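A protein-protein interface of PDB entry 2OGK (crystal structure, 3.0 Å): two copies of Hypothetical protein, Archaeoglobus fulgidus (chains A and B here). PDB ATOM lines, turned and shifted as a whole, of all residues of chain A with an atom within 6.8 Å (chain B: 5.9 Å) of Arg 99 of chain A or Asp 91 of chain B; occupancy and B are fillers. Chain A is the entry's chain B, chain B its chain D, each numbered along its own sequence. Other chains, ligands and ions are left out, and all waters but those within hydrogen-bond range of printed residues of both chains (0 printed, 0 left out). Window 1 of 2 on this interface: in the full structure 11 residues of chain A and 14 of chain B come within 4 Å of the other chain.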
ATOM      1  N   HIS A  46       5.300 -21.415 -11.509  1.00  0.00           N
ATOM      2  CA  HIS A  46       6.531 -20.708 -11.162  1.00  0.00           C
ATOM      3  C   HIS A  46       7.254 -20.146 -12.388  1.00  0.00           C
ATOM      4  O   HIS A  46       8.160 -19.299 -12.271  1.00  0.00           O
ATOM      5  CB  HIS A  46       7.461 -21.647 -10.397  1.00  0.00           C
ATOM      6  CG  HIS A  46       6.925 -22.066  -9.067  1.00  0.00           C
ATOM      7  ND1 HIS A  46       7.552 -23.001  -8.272  1.00  0.00           N
ATOM      8  CD2 HIS A  46       5.829 -21.665  -8.381  1.00  0.00           C
ATOM      9  CE1 HIS A  46       6.867 -23.157  -7.154  1.00  0.00           C
ATOM     10  NE2 HIS A  46       5.816 -22.358  -7.194  1.00  0.00           N
ATOM     11  N   LEU A  75       3.544 -40.640   7.533  1.00  0.00           N
ATOM     12  CA  LEU A  75       4.825 -39.935   7.547  1.00  0.00           C
ATOM     13  C   LEU A  75       5.886 -40.655   8.368  1.00  0.00           C
ATOM     14  O   LEU A  75       7.043 -40.758   7.951  1.00  0.00           O
ATOM     15  CB  LEU A  75       4.643 -38.514   8.097  1.00  0.00           C
ATOM     16  CG  LEU A  75       4.168 -37.457   7.092  1.00  0.00           C
ATOM     17  CD1 LEU A  75       3.535 -36.281   7.844  1.00  0.00           C
ATOM     18  CD2 LEU A  75       5.351 -37.019   6.198  1.00  0.00           C
ATOM     19  N   ARG A  89       7.425 -23.583   8.710  1.00  0.00           N
ATOM     20  CA  ARG A  89       6.205 -24.165   8.158  1.00  0.00           C
ATOM     21  C   ARG A  89       4.985 -23.380   8.607  1.00  0.00           C
ATOM     22  O   ARG A  89       3.862 -23.668   8.191  1.00  0.00           O
ATOM     23  CB  ARG A  89       6.072 -25.615   8.629  1.00  0.00           C
ATOM     24  CG  ARG A  89       7.302 -26.425   8.336  1.00  0.00           C
ATOM     25  CD  ARG A  89       7.278 -27.816   8.915  1.00  0.00           C
ATOM     26  NE  ARG A  89       8.434 -28.556   8.412  1.00  0.00           N
ATOM     27  CZ  ARG A  89       8.510 -29.099   7.199  1.00  0.00           C
ATOM     28  NH1 ARG A  89       7.495 -29.008   6.348  1.00  0.00           N
ATOM     29  NH2 ARG A  89       9.614 -29.717   6.822  1.00  0.00           N
ATOM     30  N   HIS A  97       2.410 -25.676   7.331  1.00  0.00           N
ATOM     31  CA  HIS A  97       2.695 -26.201   6.011  1.00  0.00           C
ATOM     32  C   HIS A  97       3.536 -27.452   6.030  1.00  0.00           C
ATOM     33  O   HIS A  97       4.622 -27.488   6.597  1.00  0.00           O
ATOM     34  CB  HIS A  97       3.376 -25.143   5.148  1.00  0.00           C
ATOM     35  CG  HIS A  97       2.510 -23.956   4.875  1.00  0.00           C
ATOM     36  ND1 HIS A  97       2.440 -22.874   5.726  1.00  0.00           N
ATOM     37  CD2 HIS A  97       1.623 -23.713   3.881  1.00  0.00           C
ATOM     38  CE1 HIS A  97       1.546 -22.016   5.268  1.00  0.00           C
ATOM     39  NE2 HIS A  97       1.034 -22.501   4.150  1.00  0.00           N
ATOM     40  N   ILE A  98       2.991 -28.492   5.418  1.00  0.00           N
ATOM     41  CA  ILE A  98       3.668 -29.771   5.298  1.00  0.00           C
ATOM     42  C   ILE A  98       3.682 -29.992   3.798  1.00  0.00           C
ATOM     43  O   ILE A  98       2.620 -30.135   3.185  1.00  0.00           O
ATOM     44  CB  ILE A  98       2.863 -30.950   5.924  1.00  0.00           C
ATOM     45  CG1 ILE A  98       2.485 -30.666   7.385  1.00  0.00           C
ATOM     46  CG2 ILE A  98       3.701 -32.220   5.834  1.00  0.00           C
ATOM     47  CD1 ILE A  98       3.639 -30.716   8.340  1.00  0.00           C
ATOM     48  N   ARG A  99       4.864 -30.010   3.192  1.00  0.00           N
ATOM     49  CA  ARG A  99       4.907 -30.230   1.751  1.00  0.00           C
ATOM     50  C   ARG A  99       5.255 -31.665   1.331  1.00  0.00           C
ATOM     51  O   ARG A  99       6.339 -32.183   1.604  1.00  0.00           O
ATOM     52  CB  ARG A  99       5.832 -29.209   1.099  1.00  0.00           C
ATOM     53  CG  ARG A  99       5.285 -27.801   1.237  1.00  0.00           C
ATOM     54  CD  ARG A  99       6.113 -26.840   0.435  1.00  0.00           C
ATOM     55  NE  ARG A  99       5.615 -25.468   0.468  1.00  0.00           N
ATOM     56  CZ  ARG A  99       6.234 -24.443  -0.116  1.00  0.00           C
ATOM     57  NH1 ARG A  99       7.377 -24.641  -0.776  1.00  0.00           N
ATOM     58  NH2 ARG A  99       5.711 -23.220  -0.044  1.00  0.00           N
ATOM     59  N   ILE A 100       4.290 -32.288   0.658  1.00  0.00           N
ATOM     60  CA  ILE A 100       4.404 -33.665   0.205  1.00  0.00           C
ATOM     61  C   ILE A 100       4.906 -33.893  -1.234  1.00  0.00           C
ATOM     62  O   ILE A 100       4.569 -33.163  -2.168  1.00  0.00           O
ATOM     63  CB  ILE A 100       3.035 -34.396   0.408  1.00  0.00           C
ATOM     64  CG1 ILE A 100       2.661 -34.389   1.900  1.00  0.00           C
ATOM     65  CG2 ILE A 100       3.104 -35.826  -0.102  1.00  0.00           C
ATOM     66  CD1 ILE A 100       3.786 -34.821   2.850  1.00  0.00           C
ATOM     67  N   ASP A 101       5.732 -34.924  -1.379  1.00  0.00           N
ATOM     68  CA  ASP A 101       6.313 -35.329  -2.654  1.00  0.00           C
ATOM     69  C   ASP A 101       5.245 -35.948  -3.588  1.00  0.00           C
ATOM     70  O   ASP A 101       4.801 -37.087  -3.415  1.00  0.00           O
ATOM     71  CB  ASP A 101       7.423 -36.331  -2.373  1.00  0.00           C
ATOM     72  CG  ASP A 101       8.264 -36.624  -3.577  1.00  0.00           C
ATOM     73  OD1 ASP A 101       7.710 -36.979  -4.650  1.00  0.00           O
ATOM     74  OD2 ASP A 101       9.496 -36.512  -3.428  1.00  0.00           O
ATOM     75  N   SER A 111       5.975 -39.090   1.683  1.00  0.00           N
ATOM     76  CA  SER A 111       7.285 -38.548   2.040  1.00  0.00           C
ATOM     77  C   SER A 111       7.302 -37.017   1.880  1.00  0.00           C
ATOM     78  O   SER A 111       6.482 -36.433   1.160  1.00  0.00           O
ATOM     79  CB  SER A 111       8.359 -39.182   1.146  1.00  0.00           C
ATOM     80  OG  SER A 111       9.636 -38.600   1.348  1.00  0.00           O
ATOM     81  N   LEU A 112       8.232 -36.378   2.579  1.00  0.00           N
ATOM     82  CA  LEU A 112       8.380 -34.941   2.512  1.00  0.00           C
ATOM     83  C   LEU A 112       9.161 -34.569   1.239  1.00  0.00           C
ATOM     84  O   LEU A 112       9.844 -35.425   0.643  1.00  0.00           O
ATOM     85  CB  LEU A 112       9.116 -34.445   3.760  1.00  0.00           C
ATOM     86  CG  LEU A 112       8.323 -34.452   5.074  1.00  0.00           C
ATOM     87  CD1 LEU A 112       9.194 -33.991   6.238  1.00  0.00           C
ATOM     88  CD2 LEU A 112       7.105 -33.535   4.931  1.00  0.00           C
ATOM     89  N   THR A 113       9.064 -33.304   0.824  1.00  0.00           N
ATOM     90  CA  THR A 113       9.761 -32.834  -0.368  1.00  0.00           C
ATOM     91  C   THR A 113      10.302 -31.411  -0.196  1.00  0.00           C
ATOM     92  O   THR A 113       9.634 -30.551   0.388  1.00  0.00           O
ATOM     93  CB  THR A 113       8.813 -32.881  -1.595  1.00  0.00           C
ATOM     94  OG1 THR A 113       9.489 -32.383  -2.754  1.00  0.00           O
ATOM     95  CG2 THR A 113       7.591 -32.042  -1.356  1.00  0.00           C
ATOM     96  N   SER A 114      11.511 -31.155  -0.692  1.00  0.00           N
ATOM     97  CA  SER A 114      12.100 -29.810  -0.598  1.00  0.00           C
ATOM     98  C   SER A 114      12.047 -29.052  -1.916  1.00  0.00           C
ATOM     99  O   SER A 114      12.575 -27.949  -2.015  1.00  0.00           O
ATOM    100  CB  SER A 114      13.558 -29.876  -0.141  1.00  0.00           C
ATOM    101  OG  SER A 114      13.634 -30.092   1.254  1.00  0.00           O
ATOM    102  N   GLY A 115      11.407 -29.650  -2.923  1.00  0.00           N
ATOM    103  CA  GLY A 115      11.307 -29.036  -4.240  1.00  0.00           C
ATOM    104  C   GLY A 115      10.178 -28.028  -4.392  1.00  0.00           C
ATOM    105  O   GLY A 115       9.503 -27.675  -3.408  1.00  0.00           O
ATOM    106  N   GLY A 116       9.955 -27.574  -5.624  1.00  0.00           N
ATOM    107  CA  GLY A 116       8.913 -26.596  -5.860  1.00  0.00           C
ATOM    108  C   GLY A 116       7.659 -27.044  -6.581  1.00  0.00           C
ATOM    109  O   GLY A 116       7.093 -26.272  -7.356  1.00  0.00           O
ATOM    110  N   ASP A 117       7.225 -28.282  -6.361  1.00  0.00           N
ATOM    111  CA  ASP A 117       5.999 -28.772  -6.989  1.00  0.00           C
ATOM    112  C   ASP A 117       5.424 -29.836  -6.090  1.00  0.00           C
ATOM    113  O   ASP A 117       5.101 -30.938  -6.531  1.00  0.00           O
ATOM    114  CB  ASP A 117       6.267 -29.377  -8.358  1.00  0.00           C
ATOM    115  CG  ASP A 117       4.989 -29.788  -9.070  1.00  0.00           C
ATOM    116  OD1 ASP A 117       4.146 -28.918  -9.357  1.00  0.00           O
ATOM    117  OD2 ASP A 117       4.816 -30.985  -9.349  1.00  0.00           O
ATOM    118  N   PRO A 118       5.250 -29.515  -4.803  1.00  0.00           N
ATOM    119  CA  PRO A 118       4.706 -30.551  -3.924  1.00  0.00           C
ATOM    120  C   PRO A 118       3.191 -30.600  -3.965  1.00  0.00           C
ATOM    121  O   PRO A 118       2.544 -29.936  -4.784  1.00  0.00           O
ATOM    122  CB  PRO A 118       5.214 -30.116  -2.559  1.00  0.00           C
ATOM    123  CG  PRO A 118       5.008 -28.636  -2.635  1.00  0.00           C
ATOM    124  CD  PRO A 118       5.394 -28.239  -4.076  1.00  0.00           C
ATOM    125  N   ILE A 119       2.646 -31.437  -3.098  1.00  0.00           N
ATOM    126  CA  ILE A 119       1.218 -31.543  -2.921  1.00  0.00           C
ATOM    127  C   ILE A 119       1.176 -30.799  -1.594  1.00  0.00           C
ATOM    128  O   ILE A 119       1.733 -31.262  -0.581  1.00  0.00           O
ATOM    129  CB  ILE A 119       0.767 -33.000  -2.726  1.00  0.00           C
ATOM    130  CG1 ILE A 119       0.928 -33.784  -4.023  1.00  0.00           C
ATOM    131  CG2 ILE A 119      -0.679 -33.033  -2.285  1.00  0.00           C
ATOM    132  CD1 ILE A 119       0.694 -35.253  -3.874  1.00  0.00           C
ATOM    133  N   ALA A 120       0.574 -29.618  -1.602  1.00  0.00           N
ATOM    134  CA  ALA A 120       0.518 -28.819  -0.387  1.00  0.00           C
ATOM    135  C   ALA A 120      -0.526 -29.303   0.605  1.00  0.00           C
ATOM    136  O   ALA A 120      -1.644 -29.677   0.233  1.00  0.00           O
ATOM    137  CB  ALA A 120       0.266 -27.360  -0.729  1.00  0.00           C
ATOM    138  N   VAL A 121      -0.122 -29.312   1.870  1.00  0.00           N
ATOM    139  CA  VAL A 121      -0.987 -29.686   2.977  1.00  0.00           C
ATOM    140  C   VAL A 121      -0.803 -28.571   3.987  1.00  0.00           C
ATOM    141  O   VAL A 121       0.281 -28.394   4.549  1.00  0.00           O
ATOM    142  CB  VAL A 121      -0.588 -31.031   3.601  1.00  0.00           C
ATOM    143  CG1 VAL A 121      -1.361 -31.268   4.897  1.00  0.00           C
ATOM    144  CG2 VAL A 121      -0.882 -32.144   2.605  1.00  0.00           C
ATOM    145  N   ARG B  89      15.358 -29.474  -4.764  1.00  0.00           N
ATOM    146  CA  ARG B  89      16.093 -29.019  -3.584  1.00  0.00           C
ATOM    147  C   ARG B  89      15.656 -27.640  -3.186  1.00  0.00           C
ATOM    148  O   ARG B  89      15.739 -27.274  -2.016  1.00  0.00           O
ATOM    149  CB  ARG B  89      17.586 -28.944  -3.871  1.00  0.00           C
ATOM    150  CG  ARG B  89      18.108 -30.114  -4.614  1.00  0.00           C
ATOM    151  CD  ARG B  89      19.555 -29.939  -5.009  1.00  0.00           C
ATOM    152  NE  ARG B  89      20.133 -31.266  -5.064  1.00  0.00           N
ATOM    153  CZ  ARG B  89      20.379 -31.982  -3.981  1.00  0.00           C
ATOM    154  NH1 ARG B  89      20.118 -31.475  -2.786  1.00  0.00           N
ATOM    155  NH2 ARG B  89      20.826 -33.220  -4.090  1.00  0.00           N
ATOM    156  N   ILE B  90      15.232 -26.862  -4.175  1.00  0.00           N
ATOM    157  CA  ILE B  90      14.789 -25.500  -3.926  1.00  0.00           C
ATOM    158  C   ILE B  90      13.280 -25.466  -3.742  1.00  0.00           C
ATOM    159  O   ILE B  90      12.535 -25.824  -4.646  1.00  0.00           O
ATOM    160  CB  ILE B  90      15.200 -24.564  -5.090  1.00  0.00           C
ATOM    161  CG1 ILE B  90      16.728 -24.624  -5.267  1.00  0.00           C
ATOM    162  CG2 ILE B  90      14.694 -23.136  -4.823  1.00  0.00           C
ATOM    163  CD1 ILE B  90      17.260 -23.878  -6.473  1.00  0.00           C
ATOM    164  N   ASP B  91      12.838 -25.071  -2.554  1.00  0.00           N
ATOM    165  CA  ASP B  91      11.414 -24.988  -2.297  1.00  0.00           C
ATOM    166  C   ASP B  91      10.863 -23.673  -2.794  1.00  0.00           C
ATOM    167  O   ASP B  91      11.580 -22.853  -3.348  1.00  0.00           O
ATOM    168  CB  ASP B  91      11.089 -25.142  -0.803  1.00  0.00           C
ATOM    169  CG  ASP B  91      11.903 -24.225   0.086  1.00  0.00           C
ATOM    170  OD1 ASP B  91      12.182 -23.066  -0.312  1.00  0.00           O
ATOM    171  OD2 ASP B  91      12.243 -24.680   1.201  1.00  0.00           O
ATOM    172  N   GLU B  92       9.575 -23.476  -2.580  1.00  0.00           N
ATOM    173  CA  GLU B  92       8.905 -22.272  -3.019  1.00  0.00           C
ATOM    174  C   GLU B  92       9.277 -21.031  -2.211  1.00  0.00           C
ATOM    175  O   GLU B  92       8.854 -19.928  -2.523  1.00  0.00           O
ATOM    176  CB  GLU B  92       7.402 -22.555  -3.037  1.00  0.00           C
ATOM    177  CG  GLU B  92       7.127 -23.755  -3.975  1.00  0.00           C
ATOM    178  CD  GLU B  92       5.701 -24.285  -3.958  1.00  0.00           C
ATOM    179  OE1 GLU B  92       5.063 -24.294  -5.040  1.00  0.00           O
ATOM    180  OE2 GLU B  92       5.226 -24.710  -2.878  1.00  0.00           O
ATOM    181  N   GLN B  93      10.110 -21.205  -1.195  1.00  0.00           N
ATOM    182  CA  GLN B  93      10.542 -20.074  -0.391  1.00  0.00           C
ATOM    183  C   GLN B  93      11.950 -19.754  -0.838  1.00  0.00           C
ATOM    184  O   GLN B  93      12.680 -19.038  -0.164  1.00  0.00           O
ATOM    185  CB  GLN B  93      10.530 -20.418   1.103  1.00  0.00           C
ATOM    186  CG  GLN B  93       9.304 -21.200   1.550  1.00  0.00           C
ATOM    187  CD  GLN B  93       8.012 -20.713   0.891  1.00  0.00           C
ATOM    188  OE1 GLN B  93       7.573 -19.574   1.105  1.00  0.00           O
ATOM    189  NE2 GLN B  93       7.401 -21.578   0.079  1.00  0.00           N
ATOM    190  N   ASN B  94      12.326 -20.307  -1.986  1.00  0.00           N
ATOM    191  CA  ASN B  94      13.650 -20.106  -2.574  1.00  0.00           C
ATOM    192  C   ASN B  94      14.805 -20.589  -1.722  1.00  0.00           C
ATOM    193  O   ASN B  94      15.912 -20.051  -1.800  1.00  0.00           O
ATOM    194  CB  ASN B  94      13.869 -18.645  -2.898  1.00  0.00           C
ATOM    195  CG  ASN B  94      12.794 -18.104  -3.769  1.00  0.00           C
ATOM    196  OD1 ASN B  94      12.594 -18.567  -4.897  1.00  0.00           O
ATOM    197  ND2 ASN B  94      12.067 -17.117  -3.251  1.00  0.00           N
ATOM    198  N   VAL B  95      14.559 -21.601  -0.903  1.00  0.00           N
ATOM    199  CA  VAL B  95      15.640 -22.114  -0.096  1.00  0.00           C
ATOM    200  C   VAL B  95      16.203 -23.354  -0.762  1.00  0.00           C
ATOM    201  O   VAL B  95      15.457 -24.247  -1.178  1.00  0.00           O
ATOM    202  CB  VAL B  95      15.183 -22.441   1.340  1.00  0.00           C
ATOM    203  CG1 VAL B  95      16.384 -22.835   2.178  1.00  0.00           C
ATOM    204  CG2 VAL B  95      14.502 -21.235   1.950  1.00  0.00           C
ATOM    205  N   LEU B  96      17.526 -23.364  -0.898  1.00  0.00           N
ATOM    206  CA  LEU B  96      18.239 -24.489  -1.487  1.00  0.00           C
ATOM    207  C   LEU B  96      18.655 -25.434  -0.354  1.00  0.00           C
ATOM    208  O   LEU B  96      19.372 -25.046   0.571  1.00  0.00           O
ATOM    209  CB  LEU B  96      19.457 -23.996  -2.276  1.00  0.00           C
ATOM    210  CG  LEU B  96      20.552 -24.973  -2.734  1.00  0.00           C
ATOM    211  CD1 LEU B  96      19.976 -26.185  -3.460  1.00  0.00           C
ATOM    212  CD2 LEU B  96      21.506 -24.204  -3.637  1.00  0.00           C
ATOM    213  N   HIS B  97      18.192 -26.678  -0.466  1.00  0.00           N
ATOM    214  CA  HIS B  97      18.418 -27.722   0.523  1.00  0.00           C
ATOM    215  C   HIS B  97      19.445 -28.798   0.205  1.00  0.00           C
ATOM    216  O   HIS B  97      19.374 -29.475  -0.821  1.00  0.00           O
ATOM    217  CB  HIS B  97      17.091 -28.387   0.815  1.00  0.00           C
ATOM    218  CG  HIS B  97      16.055 -27.436   1.305  1.00  0.00           C
ATOM    219  ND1 HIS B  97      16.047 -26.956   2.592  1.00  0.00           N
ATOM    220  CD2 HIS B  97      15.004 -26.861   0.679  1.00  0.00           C
ATOM    221  CE1 HIS B  97      15.032 -26.127   2.743  1.00  0.00           C
ATOM    222  NE2 HIS B  97      14.382 -26.051   1.597  1.00  0.00           N
ATOM    223  N   ARG B 132      11.100 -17.969  -9.663  1.00  0.00           N
ATOM    224  CA  ARG B 132      11.605 -19.337  -9.638  1.00  0.00           C
ATOM    225  C   ARG B 132      12.682 -19.390 -10.715  1.00  0.00           C
ATOM    226  O   ARG B 132      13.768 -19.950 -10.532  1.00  0.00           O
ATOM    227  CB  ARG B 132      10.469 -20.300  -9.993  1.00  0.00           C
ATOM    228  CG  ARG B 132      10.835 -21.767 -10.062  1.00  0.00           C
ATOM    229  CD  ARG B 132      11.071 -22.301  -8.698  1.00  0.00           C
ATOM    230  NE  ARG B 132      11.349 -23.733  -8.670  1.00  0.00           N
ATOM    231  CZ  ARG B 132      11.531 -24.432  -7.550  1.00  0.00           C
ATOM    232  NH1 ARG B 132      11.452 -23.825  -6.373  1.00  0.00           N
ATOM    233  NH2 ARG B 132      11.828 -25.727  -7.599  1.00  0.00           N
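Printed residues of chain A that touch a printed residue of chain B: His 46, Arg 99, Ser 114, Gly 115, Gly 116 and Pro 118. Along chain A the printed residues that touch a printed residue of chain B span positions 46 to 118. Among the printed residues, Asp or Glu carboxylates within 4 Å of a Lys or Arg side-chain nitrogen of the other chain: Arg 99 of chain A with Glu 92 of chain B (3.0 Å).
O of Ile 90 of chain B sits close to O of Ser 114 of chain A, at 3.4 Å. The guanidinium group of Arg 132 of chain B sits close to the backbone NH of Gly 116 of chain A (3.3 Å). The guanidinium group of Arg 99 of chain A lies within salt-bridge range of the side-chain carboxylate of Glu 92 of chain B (3.0 Å). NE2 of His 46 of chain A is in hydrogen-bond range of OE1 of Glu 92 of chain B. O of Ser 114 of chain A sits close to O of Arg 89 of chain B, at 3.2 Å. The backbone carbonyl oxygen (O) of Ser 114 of chain A lies within hydrogen-bond range of the backbone NH (N) of Asp 91 of chain B (2.9 Å). N of Gly 116 of chain A sits at hydrogen-bond distance from O of Ile 90 of chain B, 3.3 Å away. The side-chain amide nitrogen (NE2) of Gln 93 of chain B lies close to the guanidinium group (NH1) of Arg 99 of chain A (3.2 Å).
Arg 132 of chain B touches His 46 of chain A. Asp 91 of chain B touches Arg 99 of chain A. Ser 114 of chain A touches His 97 of chain B. Ile 90 of chain B touches Gly 115 of chain A (O to C, 3.2 Å). Gly 115 of chain A touches Asp 91 of chain B. O of Gly 116 of chain A touches OE1 of Glu 92 of chain B, at 3.7 Å. OE2 of Glu 92 of chain B touches CD of Pro 118 of chain A, at 3.7 Å.
2 positions are printed for both chains.
The backbone carbonyl oxygen (O) of His 97 of chain B is in hydrogen-bond range of the guanidinium group (NH1) of Arg 89 of chain B (2.9 Å). OD1 of Asp 91 of chain B lies within hydrogen-bond range of N of Asn 94 of chain B (3.2 Å). The backbone carbonyl oxygen (O) of Gly 116 of chain A sits close to a ring nitrogen (ND1) of His 46 of chain A (3.4 Å). N of Val 95 of chain B sits at hydrogen-bond distance from OD1 of Asp 91 of chain B (2.9 Å). The side-chain carboxylate (OD1) of Asp 91 of chain B lies within hydrogen-bond range of the backbone NH (N) of Gln 93 of chain B, 2.9 Å away. OD2 of Asp 91 of chain B lies within hydrogen-bond range of NE2 of His 97 of chain B, at 2.6 Å.
Arg 99 of chain A touches just these residues of chain B: Asp 91, Glu 92 and Gln 93. Printed residues of chain B within 4 Å of Ser 114 of chain A: Arg 89 (3.2 Å), Ile 90 (3.1 Å), Asp 91 (2.9 Å) and His 97 (3.4 Å). Printed residues of chain A within 4 Å of Glu 92 of chain B: His 46, Arg 99, Gly 116 and Pro 118. Of the printed residues of chain A, His 97 of chain B touches Ser 114. Printed residues of chain A within 4 Å of Arg 132 of chain B: His 46 and Gly 116. The nearest printed residue of chain A that does not touch Glu 92 of chain B is Gly 115 of chain A (4.3 Å).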
